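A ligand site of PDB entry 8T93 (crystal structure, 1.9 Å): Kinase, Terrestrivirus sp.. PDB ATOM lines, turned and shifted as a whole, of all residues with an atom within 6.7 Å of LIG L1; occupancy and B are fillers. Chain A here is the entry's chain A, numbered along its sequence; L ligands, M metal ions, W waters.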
ATOM      1  N   ALA A  40     -25.557  21.095 -13.121  1.00  0.00           N
ATOM      2  CA  ALA A  40     -26.433  20.415 -14.107  1.00  0.00           C
ATOM      3  C   ALA A  40     -25.615  19.758 -15.231  1.00  0.00           C
ATOM      4  O   ALA A  40     -24.357  19.799 -15.155  1.00  0.00           O
ATOM      5  CB  ALA A  40     -27.434  21.413 -14.654  1.00  0.00           C
ATOM      6  N   GLY A  41     -26.296  19.211 -16.232  1.00  0.00           N
ATOM      7  CA  GLY A  41     -25.670  18.599 -17.432  1.00  0.00           C
ATOM      8  C   GLY A  41     -25.094  17.227 -17.091  1.00  0.00           C
ATOM      9  O   GLY A  41     -25.291  16.781 -15.995  1.00  0.00           O
ATOM     10  N   ARG A  42     -24.368  16.584 -18.007  1.00  0.00           N
ATOM     11  CA  ARG A  42     -23.989  15.145 -17.926  1.00  0.00           C
ATOM     12  C   ARG A  42     -22.496  14.934 -18.223  1.00  0.00           C
ATOM     13  O   ARG A  42     -21.994  13.795 -18.032  1.00  0.00           O
ATOM     14  CB  ARG A  42     -24.776  14.320 -18.960  1.00  0.00           C
ATOM     15  CG  ARG A  42     -26.278  14.350 -18.784  1.00  0.00           C
ATOM     16  CD  ARG A  42     -26.962  13.177 -19.496  1.00  0.00           C
ATOM     17  NE  ARG A  42     -28.410  13.299 -19.296  1.00  0.00           N
ATOM     18  CZ  ARG A  42     -29.340  12.661 -20.004  1.00  0.00           C
ATOM     19  NH1 ARG A  42     -28.997  11.833 -20.978  1.00  0.00           N
ATOM     20  NH2 ARG A  42     -30.627  12.857 -19.739  1.00  0.00           N
ATOM     21  N   SER A  43     -21.788  15.975 -18.679  1.00  0.00           N
ATOM     22  CA  SER A  43     -20.381  15.840 -19.118  1.00  0.00           C
ATOM     23  C   SER A  43     -19.515  15.580 -17.902  1.00  0.00           C
ATOM     24  O   SER A  43     -19.844  16.039 -16.827  1.00  0.00           O
ATOM     25  CB  SER A  43     -19.898  17.039 -19.919  1.00  0.00           C
ATOM     26  OG  SER A  43     -20.571  17.079 -21.173  1.00  0.00           O
ATOM     27  N   LYS A  60     -19.005  13.569 -27.432  1.00  0.00           N
ATOM     28  CA  LYS A  60     -19.532  12.931 -28.690  1.00  0.00           C
ATOM     29  C   LYS A  60     -18.825  13.450 -29.932  1.00  0.00           C
ATOM     30  O   LYS A  60     -18.747  12.734 -30.950  1.00  0.00           O
ATOM     31  CB  LYS A  60     -20.999  13.333 -28.804  1.00  0.00           C
ATOM     32  CG  LYS A  60     -21.778  12.933 -27.570  1.00  0.00           C
ATOM     33  CD  LYS A  60     -23.156  13.482 -27.447  1.00  0.00           C
ATOM     34  CE  LYS A  60     -23.610  13.153 -26.053  1.00  0.00           C
ATOM     35  NZ  LYS A  60     -25.043  13.374 -25.871  1.00  0.00           N
ATOM     36  N   ASP A 110     -27.672  27.215 -12.917  1.00  0.00           N
ATOM     37  CA  ASP A 110     -27.552  26.886 -14.338  1.00  0.00           C
ATOM     38  C   ASP A 110     -28.937  27.111 -14.939  1.00  0.00           C
ATOM     39  O   ASP A 110     -29.875  26.384 -14.522  1.00  0.00           O
ATOM     40  CB  ASP A 110     -27.049  25.459 -14.540  1.00  0.00           C
ATOM     41  CG  ASP A 110     -26.868  25.023 -16.000  1.00  0.00           C
ATOM     42  OD1 ASP A 110     -27.633  25.462 -16.875  1.00  0.00           O
ATOM     43  OD2 ASP A 110     -25.951  24.220 -16.245  1.00  0.00           O
ATOM     44  N   LYS A 112     -30.755  27.058 -18.648  1.00  0.00           N
ATOM     45  CA  LYS A 112     -30.652  26.779 -20.099  1.00  0.00           C
ATOM     46  C   LYS A 112     -31.453  27.845 -20.840  1.00  0.00           C
ATOM     47  O   LYS A 112     -32.643  27.908 -20.627  1.00  0.00           O
ATOM     48  CB  LYS A 112     -31.048  25.352 -20.476  1.00  0.00           C
ATOM     49  CG  LYS A 112     -30.831  25.026 -21.938  1.00  0.00           C
ATOM     50  CD  LYS A 112     -30.925  23.584 -22.280  1.00  0.00           C
ATOM     51  CE  LYS A 112     -29.957  22.691 -21.545  1.00  0.00           C
ATOM     52  NZ  LYS A 112     -30.048  21.286 -21.998  1.00  0.00           N
ATOM     53  N   ALA A 115     -32.172  26.606 -27.169  1.00  0.00           N
ATOM     54  CA  ALA A 115     -33.185  25.558 -27.439  1.00  0.00           C
ATOM     55  C   ALA A 115     -32.742  24.275 -26.778  1.00  0.00           C
ATOM     56  O   ALA A 115     -31.545  23.940 -26.798  1.00  0.00           O
ATOM     57  CB  ALA A 115     -33.449  25.386 -28.923  1.00  0.00           C
ATOM     58  N   ARG A 116     -33.688  23.571 -26.198  1.00  0.00           N
ATOM     59  CA  ARG A 116     -33.485  22.185 -25.734  1.00  0.00           C
ATOM     60  C   ARG A 116     -33.570  21.267 -26.951  1.00  0.00           C
ATOM     61  O   ARG A 116     -33.936  21.749 -28.048  1.00  0.00           O
ATOM     62  CB  ARG A 116     -34.562  21.827 -24.709  1.00  0.00           C
ATOM     63  CG  ARG A 116     -34.705  22.839 -23.586  1.00  0.00           C
ATOM     64  CD  ARG A 116     -35.749  22.417 -22.581  1.00  0.00           C
ATOM     65  NE  ARG A 116     -35.234  21.377 -21.708  1.00  0.00           N
ATOM     66  CZ  ARG A 116     -35.939  20.689 -20.809  1.00  0.00           C
ATOM     67  NH1 ARG A 116     -37.234  20.891 -20.643  1.00  0.00           N
ATOM     68  NH2 ARG A 116     -35.307  19.783 -20.095  1.00  0.00           N
ATOM     69  N   LYS A 117     -33.147  20.007 -26.781  1.00  0.00           N
ATOM     70  CA  LYS A 117     -33.041  19.039 -27.875  1.00  0.00           C
ATOM     71  C   LYS A 117     -34.456  18.760 -28.404  1.00  0.00           C
ATOM     72  O   LYS A 117     -34.672  18.990 -29.587  1.00  0.00           O
ATOM     73  CB  LYS A 117     -32.303  17.796 -27.382  1.00  0.00           C
ATOM     74  CG  LYS A 117     -30.882  17.595 -27.894  1.00  0.00           C
ATOM     75  CD  LYS A 117     -30.736  16.263 -28.621  1.00  0.00           C
ATOM     76  CE  LYS A 117     -29.367  15.647 -28.588  1.00  0.00           C
ATOM     77  NZ  LYS A 117     -29.219  14.724 -27.451  1.00  0.00           N
ATOM     78  N   ARG A 118     -35.394  18.397 -27.539  1.00  0.00           N
ATOM     79  CA  ARG A 118     -36.779  18.088 -27.994  1.00  0.00           C
ATOM     80  C   ARG A 118     -37.827  18.857 -27.187  1.00  0.00           C
ATOM     81  O   ARG A 118     -38.710  19.459 -27.793  1.00  0.00           O
ATOM     82  CB  ARG A 118     -37.059  16.609 -27.735  1.00  0.00           C
ATOM     83  CG  ARG A 118     -36.488  15.663 -28.767  1.00  0.00           C
ATOM     84  CD  ARG A 118     -35.037  15.363 -28.488  1.00  0.00           C
ATOM     85  NE  ARG A 118     -34.340  14.711 -29.582  1.00  0.00           N
ATOM     86  CZ  ARG A 118     -33.563  13.653 -29.434  1.00  0.00           C
ATOM     87  NH1 ARG A 118     -33.401  13.149 -28.226  1.00  0.00           N
ATOM     88  NH2 ARG A 118     -32.952  13.100 -30.463  1.00  0.00           N
ATOM     89  N   LYS A 119     -37.709  18.823 -25.869  1.00  0.00           N
ATOM     90  CA  LYS A 119     -38.697  19.367 -24.913  1.00  0.00           C
ATOM     91  C   LYS A 119     -38.810  20.883 -25.101  1.00  0.00           C
ATOM     92  O   LYS A 119     -37.862  21.543 -25.556  1.00  0.00           O
ATOM     93  CB  LYS A 119     -38.278  18.983 -23.503  1.00  0.00           C
ATOM     94  CG  LYS A 119     -38.018  17.496 -23.329  1.00  0.00           C
ATOM     95  CD  LYS A 119     -37.527  17.133 -21.955  1.00  0.00           C
ATOM     96  CE  LYS A 119     -37.998  15.767 -21.498  1.00  0.00           C
ATOM     97  NZ  LYS A 119     -37.086  15.234 -20.458  1.00  0.00           N
ATOM     98  N   SER A 120     -39.988  21.397 -24.787  1.00  0.00           N
ATOM     99  CA  SER A 120     -40.205  22.814 -24.463  1.00  0.00           C
ATOM    100  C   SER A 120     -39.495  23.150 -23.123  1.00  0.00           C
ATOM    101  O   SER A 120     -39.201  22.263 -22.282  1.00  0.00           O
ATOM    102  CB  SER A 120     -41.684  23.104 -24.446  1.00  0.00           C
ATOM    103  OG  SER A 120     -42.297  22.439 -23.348  1.00  0.00           O
ATOM    104  N   HIS A 121     -39.283  24.436 -22.913  1.00  0.00           N
ATOM    105  CA  HIS A 121     -38.655  24.980 -21.691  1.00  0.00           C
ATOM    106  C   HIS A 121     -39.618  24.811 -20.522  1.00  0.00           C
ATOM    107  O   HIS A 121     -40.833  25.058 -20.725  1.00  0.00           O
ATOM    108  CB  HIS A 121     -38.264  26.445 -21.932  1.00  0.00           C
ATOM    109  CG  HIS A 121     -36.981  26.593 -22.677  1.00  0.00           C
ATOM    110  ND1 HIS A 121     -35.826  25.987 -22.253  1.00  0.00           N
ATOM    111  CD2 HIS A 121     -36.668  27.280 -23.791  1.00  0.00           C
ATOM    112  CE1 HIS A 121     -34.837  26.308 -23.063  1.00  0.00           C
ATOM    113  NE2 HIS A 121     -35.317  27.110 -24.007  1.00  0.00           N
ATOM    114  N   SER A 127     -35.227  27.245 -19.035  1.00  0.00           N
ATOM    115  CA  SER A 127     -35.347  26.150 -18.046  1.00  0.00           C
ATOM    116  C   SER A 127     -34.249  26.310 -17.002  1.00  0.00           C
ATOM    117  O   SER A 127     -33.029  26.075 -17.344  1.00  0.00           O
ATOM    118  CB  SER A 127     -35.252  24.814 -18.714  1.00  0.00           C
ATOM    119  OG  SER A 127     -36.149  24.775 -19.811  1.00  0.00           O
ATOM    120  N   ARG A 129     -31.977  24.665 -14.732  1.00  0.00           N
ATOM    121  CA  ARG A 129     -31.477  23.268 -14.730  1.00  0.00           C
ATOM    122  C   ARG A 129     -31.025  22.823 -13.332  1.00  0.00           C
ATOM    123  O   ARG A 129     -30.987  21.641 -13.107  1.00  0.00           O
ATOM    124  CB  ARG A 129     -30.376  23.051 -15.769  1.00  0.00           C
ATOM    125  CG  ARG A 129     -30.795  23.340 -17.195  1.00  0.00           C
ATOM    126  CD  ARG A 129     -32.282  23.104 -17.423  1.00  0.00           C
ATOM    127  NE  ARG A 129     -32.629  21.709 -17.482  1.00  0.00           N
ATOM    128  CZ  ARG A 129     -33.737  21.139 -17.039  1.00  0.00           C
ATOM    129  NH1 ARG A 129     -33.924  19.867 -17.202  1.00  0.00           N
ATOM    130  NH2 ARG A 129     -34.645  21.864 -16.441  1.00  0.00           N
ATOM    131  N   GLY A 195     -28.807  24.675 -26.663  1.00  0.00           N
ATOM    132  CA  GLY A 195     -28.308  23.984 -25.463  1.00  0.00           C
ATOM    133  C   GLY A 195     -27.449  24.879 -24.570  1.00  0.00           C
ATOM    134  O   GLY A 195     -26.980  24.366 -23.523  1.00  0.00           O
ATOM    135  N   SER A 197     -26.208  27.515 -21.709  1.00  0.00           N
ATOM    136  CA  SER A 197     -26.685  27.884 -20.361  1.00  0.00           C
ATOM    137  C   SER A 197     -26.031  29.189 -19.871  1.00  0.00           C
ATOM    138  O   SER A 197     -24.951  29.498 -20.307  1.00  0.00           O
ATOM    139  CB  SER A 197     -26.365  26.798 -19.357  1.00  0.00           C
ATOM    140  OG  SER A 197     -27.289  25.760 -19.348  1.00  0.00           O
ATOM    141  N   ASP A 215     -21.301  26.111 -22.496  1.00  0.00           N
ATOM    142  CA  ASP A 215     -21.775  24.868 -23.122  1.00  0.00           C
ATOM    143  C   ASP A 215     -22.097  25.122 -24.574  1.00  0.00           C
ATOM    144  O   ASP A 215     -23.286  25.294 -24.911  1.00  0.00           O
ATOM    145  CB  ASP A 215     -23.018  24.282 -22.456  1.00  0.00           C
ATOM    146  CG  ASP A 215     -23.240  22.835 -22.882  1.00  0.00           C
ATOM    147  OD1 ASP A 215     -22.512  22.410 -23.841  1.00  0.00           O
ATOM    148  OD2 ASP A 215     -24.115  22.148 -22.229  1.00  0.00           O
ATOM    149  N   ARG A 218     -23.669  22.106 -28.703  1.00  0.00           N
ATOM    150  CA  ARG A 218     -24.717  21.946 -29.761  1.00  0.00           C
ATOM    151  C   ARG A 218     -24.895  23.217 -30.591  1.00  0.00           C
ATOM    152  O   ARG A 218     -25.881  23.366 -31.344  1.00  0.00           O
ATOM    153  CB  ARG A 218     -26.022  21.481 -29.106  1.00  0.00           C
ATOM    154  CG  ARG A 218     -25.950  20.070 -28.536  1.00  0.00           C
ATOM    155  CD  ARG A 218     -27.317  19.377 -28.540  1.00  0.00           C
ATOM    156  NE  ARG A 218     -28.238  20.172 -27.742  1.00  0.00           N
ATOM    157  CZ  ARG A 218     -29.322  20.876 -28.168  1.00  0.00           C
ATOM    158  NH1 ARG A 218     -29.739  20.876 -29.448  1.00  0.00           N
ATOM    159  NH2 ARG A 218     -30.021  21.569 -27.262  1.00  0.00           N
HETATM  160  O1  LIG L   1     -27.638  17.199 -20.029  1.00  0.00           O
HETATM  161  P1  LIG L   1     -28.935  18.144 -20.316  1.00  0.00           P
HETATM  162  O2  LIG L   1     -29.890  18.057 -19.170  1.00  0.00           O
HETATM  163  O3  LIG L   1     -28.355  19.708 -20.418  1.00  0.00           O
HETATM  164  O4  LIG L   1     -29.652  17.871 -21.842  1.00  0.00           O
HETATM  165  C1  LIG L   1     -30.141  16.637 -22.126  1.00  0.00           C
HETATM  166  C2  LIG L   1     -31.253  16.870 -22.999  1.00  0.00           C
HETATM  167  O5  LIG L   1     -32.154  17.691 -22.235  1.00  0.00           O
HETATM  168  P2  LIG L   1     -32.798  18.959 -22.983  1.00  0.00           P
HETATM  169  O6  LIG L   1     -32.024  19.403 -24.362  1.00  0.00           O
HETATM  170  O7  LIG L   1     -34.269  18.619 -23.085  1.00  0.00           O
HETATM  171  O8  LIG L   1     -32.528  20.308 -21.897  1.00  0.00           O
HETATM  172  C3  LIG L   1     -32.060  15.622 -23.326  1.00  0.00           C
HETATM  173  O9  LIG L   1     -32.903  16.065 -24.337  1.00  0.00           O
HETATM  174  P3  LIG L   1     -34.465  15.750 -24.506  1.00  0.00           P
HETATM  175  O10 LIG L   1     -35.164  17.100 -25.162  1.00  0.00           O
HETATM  176  O11 LIG L   1     -34.328  14.637 -25.685  1.00  0.00           O
HETATM  177  O12 LIG L   1     -34.919  15.195 -23.184  1.00  0.00           O
HETATM  178  C4  LIG L   1     -29.056  15.725 -22.750  1.00  0.00           C
HETATM  179  O13 LIG L   1     -27.980  15.265 -21.741  1.00  0.00           O
HETATM  180  C5  LIG L   1     -29.881  14.388 -23.063  1.00  0.00           C
HETATM  181  O14 LIG L   1     -28.972  13.481 -23.611  1.00  0.00           O
HETATM  182  C6  LIG L   1     -31.091  14.582 -23.956  1.00  0.00           C
HETATM  183  O15 LIG L   1     -31.853  13.308 -24.180  1.00  0.00           O
HETATM  184  P4  LIG L   1     -31.471  12.308 -25.413  1.00  0.00           P
HETATM  185  O16 LIG L   1     -31.123  13.178 -26.602  1.00  0.00           O
HETATM  186  O17 LIG L   1     -32.698  11.193 -25.565  1.00  0.00           O
HETATM  187  O18 LIG L   1     -30.206  11.378 -24.817  1.00  0.00           O
HETATM  188  P1  LG2 L   2     -22.820  19.868 -19.984  1.00  0.00           P
HETATM  189  O1  LG2 L   2     -24.274  20.335 -19.930  1.00  0.00           O
HETATM  190  O2  LG2 L   2     -22.464  18.764 -19.095  1.00  0.00           O
HETATM  191  O3  LG2 L   2     -22.341  19.698 -21.519  1.00  0.00           O
HETATM  192  P2  LG2 L   2     -22.033  22.609 -19.175  1.00  0.00           P
HETATM  193  O4  LG2 L   2     -23.461  22.974 -19.417  1.00  0.00           O
HETATM  194  O5  LG2 L   2     -20.922  23.383 -19.850  1.00  0.00           O
HETATM  195  O6  LG2 L   2     -21.784  21.051 -19.456  1.00  0.00           O
HETATM  196  O7  LG2 L   2     -21.733  22.658 -17.602  1.00  0.00           O
HETATM  197  C1  LG2 L   2     -22.342  21.740 -16.653  1.00  0.00           C
HETATM  198  C2  LG2 L   2     -22.138  22.329 -15.285  1.00  0.00           C
HETATM  199  O8  LG2 L   2     -20.727  22.572 -15.065  1.00  0.00           O
HETATM  200  C3  LG2 L   2     -22.783  23.708 -15.063  1.00  0.00           C
HETATM  201  O9  LG2 L   2     -24.112  23.567 -14.565  1.00  0.00           O
HETATM  202  C4  LG2 L   2     -21.861  24.339 -14.007  1.00  0.00           C
HETATM  203  O10 LG2 L   2     -22.214  23.907 -12.709  1.00  0.00           O
HETATM  204  C5  LG2 L   2     -20.498  23.768 -14.357  1.00  0.00           C
HETATM  205  N1  LG2 L   2     -19.643  24.612 -15.200  1.00  0.00           N
HETATM  206  C6  LG2 L   2     -19.445  24.561 -16.565  1.00  0.00           C
HETATM  207  N2  LG2 L   2     -18.529  25.406 -17.004  1.00  0.00           N
HETATM  208  C7  LG2 L   2     -18.047  25.981 -15.847  1.00  0.00           C
HETATM  209  C8  LG2 L   2     -17.038  26.912 -15.648  1.00  0.00           C
HETATM  210  N3  LG2 L   2     -16.282  27.395 -16.665  1.00  0.00           N
HETATM  211  N4  LG2 L   2     -16.788  27.249 -14.368  1.00  0.00           N
HETATM  212  C9  LG2 L   2     -17.514  26.711 -13.376  1.00  0.00           C
HETATM  213  N5  LG2 L   2     -18.521  25.833 -13.433  1.00  0.00           N
HETATM  214  C10 LG2 L   2     -18.732  25.505 -14.720  1.00  0.00           C
HETATM  215 MG    MG M   1     -25.064  22.189 -20.346  1.00  0.00          MG
HETATM  216  O   HOH W   1     -27.067  10.471 -24.868  1.00  0.00           O
HETATM  217  O   HOH W   2     -29.841  20.594 -24.782  1.00  0.00           O
HETATM  218  O   HOH W   3     -31.611  20.006 -19.568  1.00  0.00           O
HETATM  219  O   HOH W   4     -29.264  19.337 -16.879  1.00  0.00           O
HETATM  220  O   HOH W   5     -28.538  21.211 -18.256  1.00  0.00           O
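N of Arg 42 sits at hydrogen-bond distance from O2 of LG2 L2, at 3.1 Å.
The side-chain carboxylate (OD2) of Asp 110 is in hydrogen-bond range of an oxygen (O9) of LG2 L2 (2.6 Å).
The backbone NH of Lys 119 lies within hydrogen-bond range of an oxygen (O10) of LIG L1 (3.2 Å).
N of Arg 118 is in hydrogen-bond range of O10 of LIG L1 (2.7 Å).
O3 of LG2 L2 is in hydrogen-bond range of OG of Ser 43, at 3.2 Å.
The guanidinium group (NH1) of Arg 42 sits at hydrogen-bond distance from an oxygen (O14) of LIG L1 (3.1 Å).
NZ of Lys 117 is in salt-bridge range of O16 of LIG L1, at 2.6 Å.
N of Ala 40 lies within hydrogen-bond range of O9 of LG2 L2 (3.2 Å).
An oxygen (O12) of LIG L1 is in salt-bridge range of the side-chain amino group (NZ) of Lys 119 (3.5 Å).
An oxygen (O2) of LG2 L2 is in hydrogen-bond range of the backbone NH (N) of Ser 43 (2.9 Å).
An oxygen (O8) of LIG L1 is in salt-bridge range of the side-chain amino group (NZ) of Lys 112 (2.7 Å).
The guanidinium group (NH1) of Arg 118 lies within salt-bridge range of an oxygen (O16) of LIG L1 (2.8 Å).
NE of Arg 116 is in salt-bridge range of O8 of LIG L1 (2.9 Å).
An oxygen (O6) of LIG L1 is in hydrogen-bond range of the backbone NH (N) of Lys 117, 2.7 Å away.
The guanidinium group (NH1) of Arg 116 sits at hydrogen-bond distance from the backbone carbonyl oxygen (O) of Ser 120, at 2.9 Å.
The backbone carbonyl oxygen (O) of Ser 127 sits at hydrogen-bond distance from the backbone NH (N) of Lys 112, at 2.8 Å.
Gly 41 touches LIG L1.
Of the 20 residues printed, 7 come within 4 Å of LIG L1.
Water W3 lies within hydrogen-bond range of an oxygen (O8) of LIG L1 (2.5 Å), the guanidinium group of Arg 129 (2.9 Å) and the side-chain amino group of Lys 112 (3.2 Å).
Water W2 lies within hydrogen-bond range of O6 of LIG L1, NH2 of Arg 218 and NZ of Lys 112.
Water W4 bridges an oxygen (O2) of LIG L1 (2.7 Å) and the backbone NH (N) of Gly 41 (3.0 Å).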
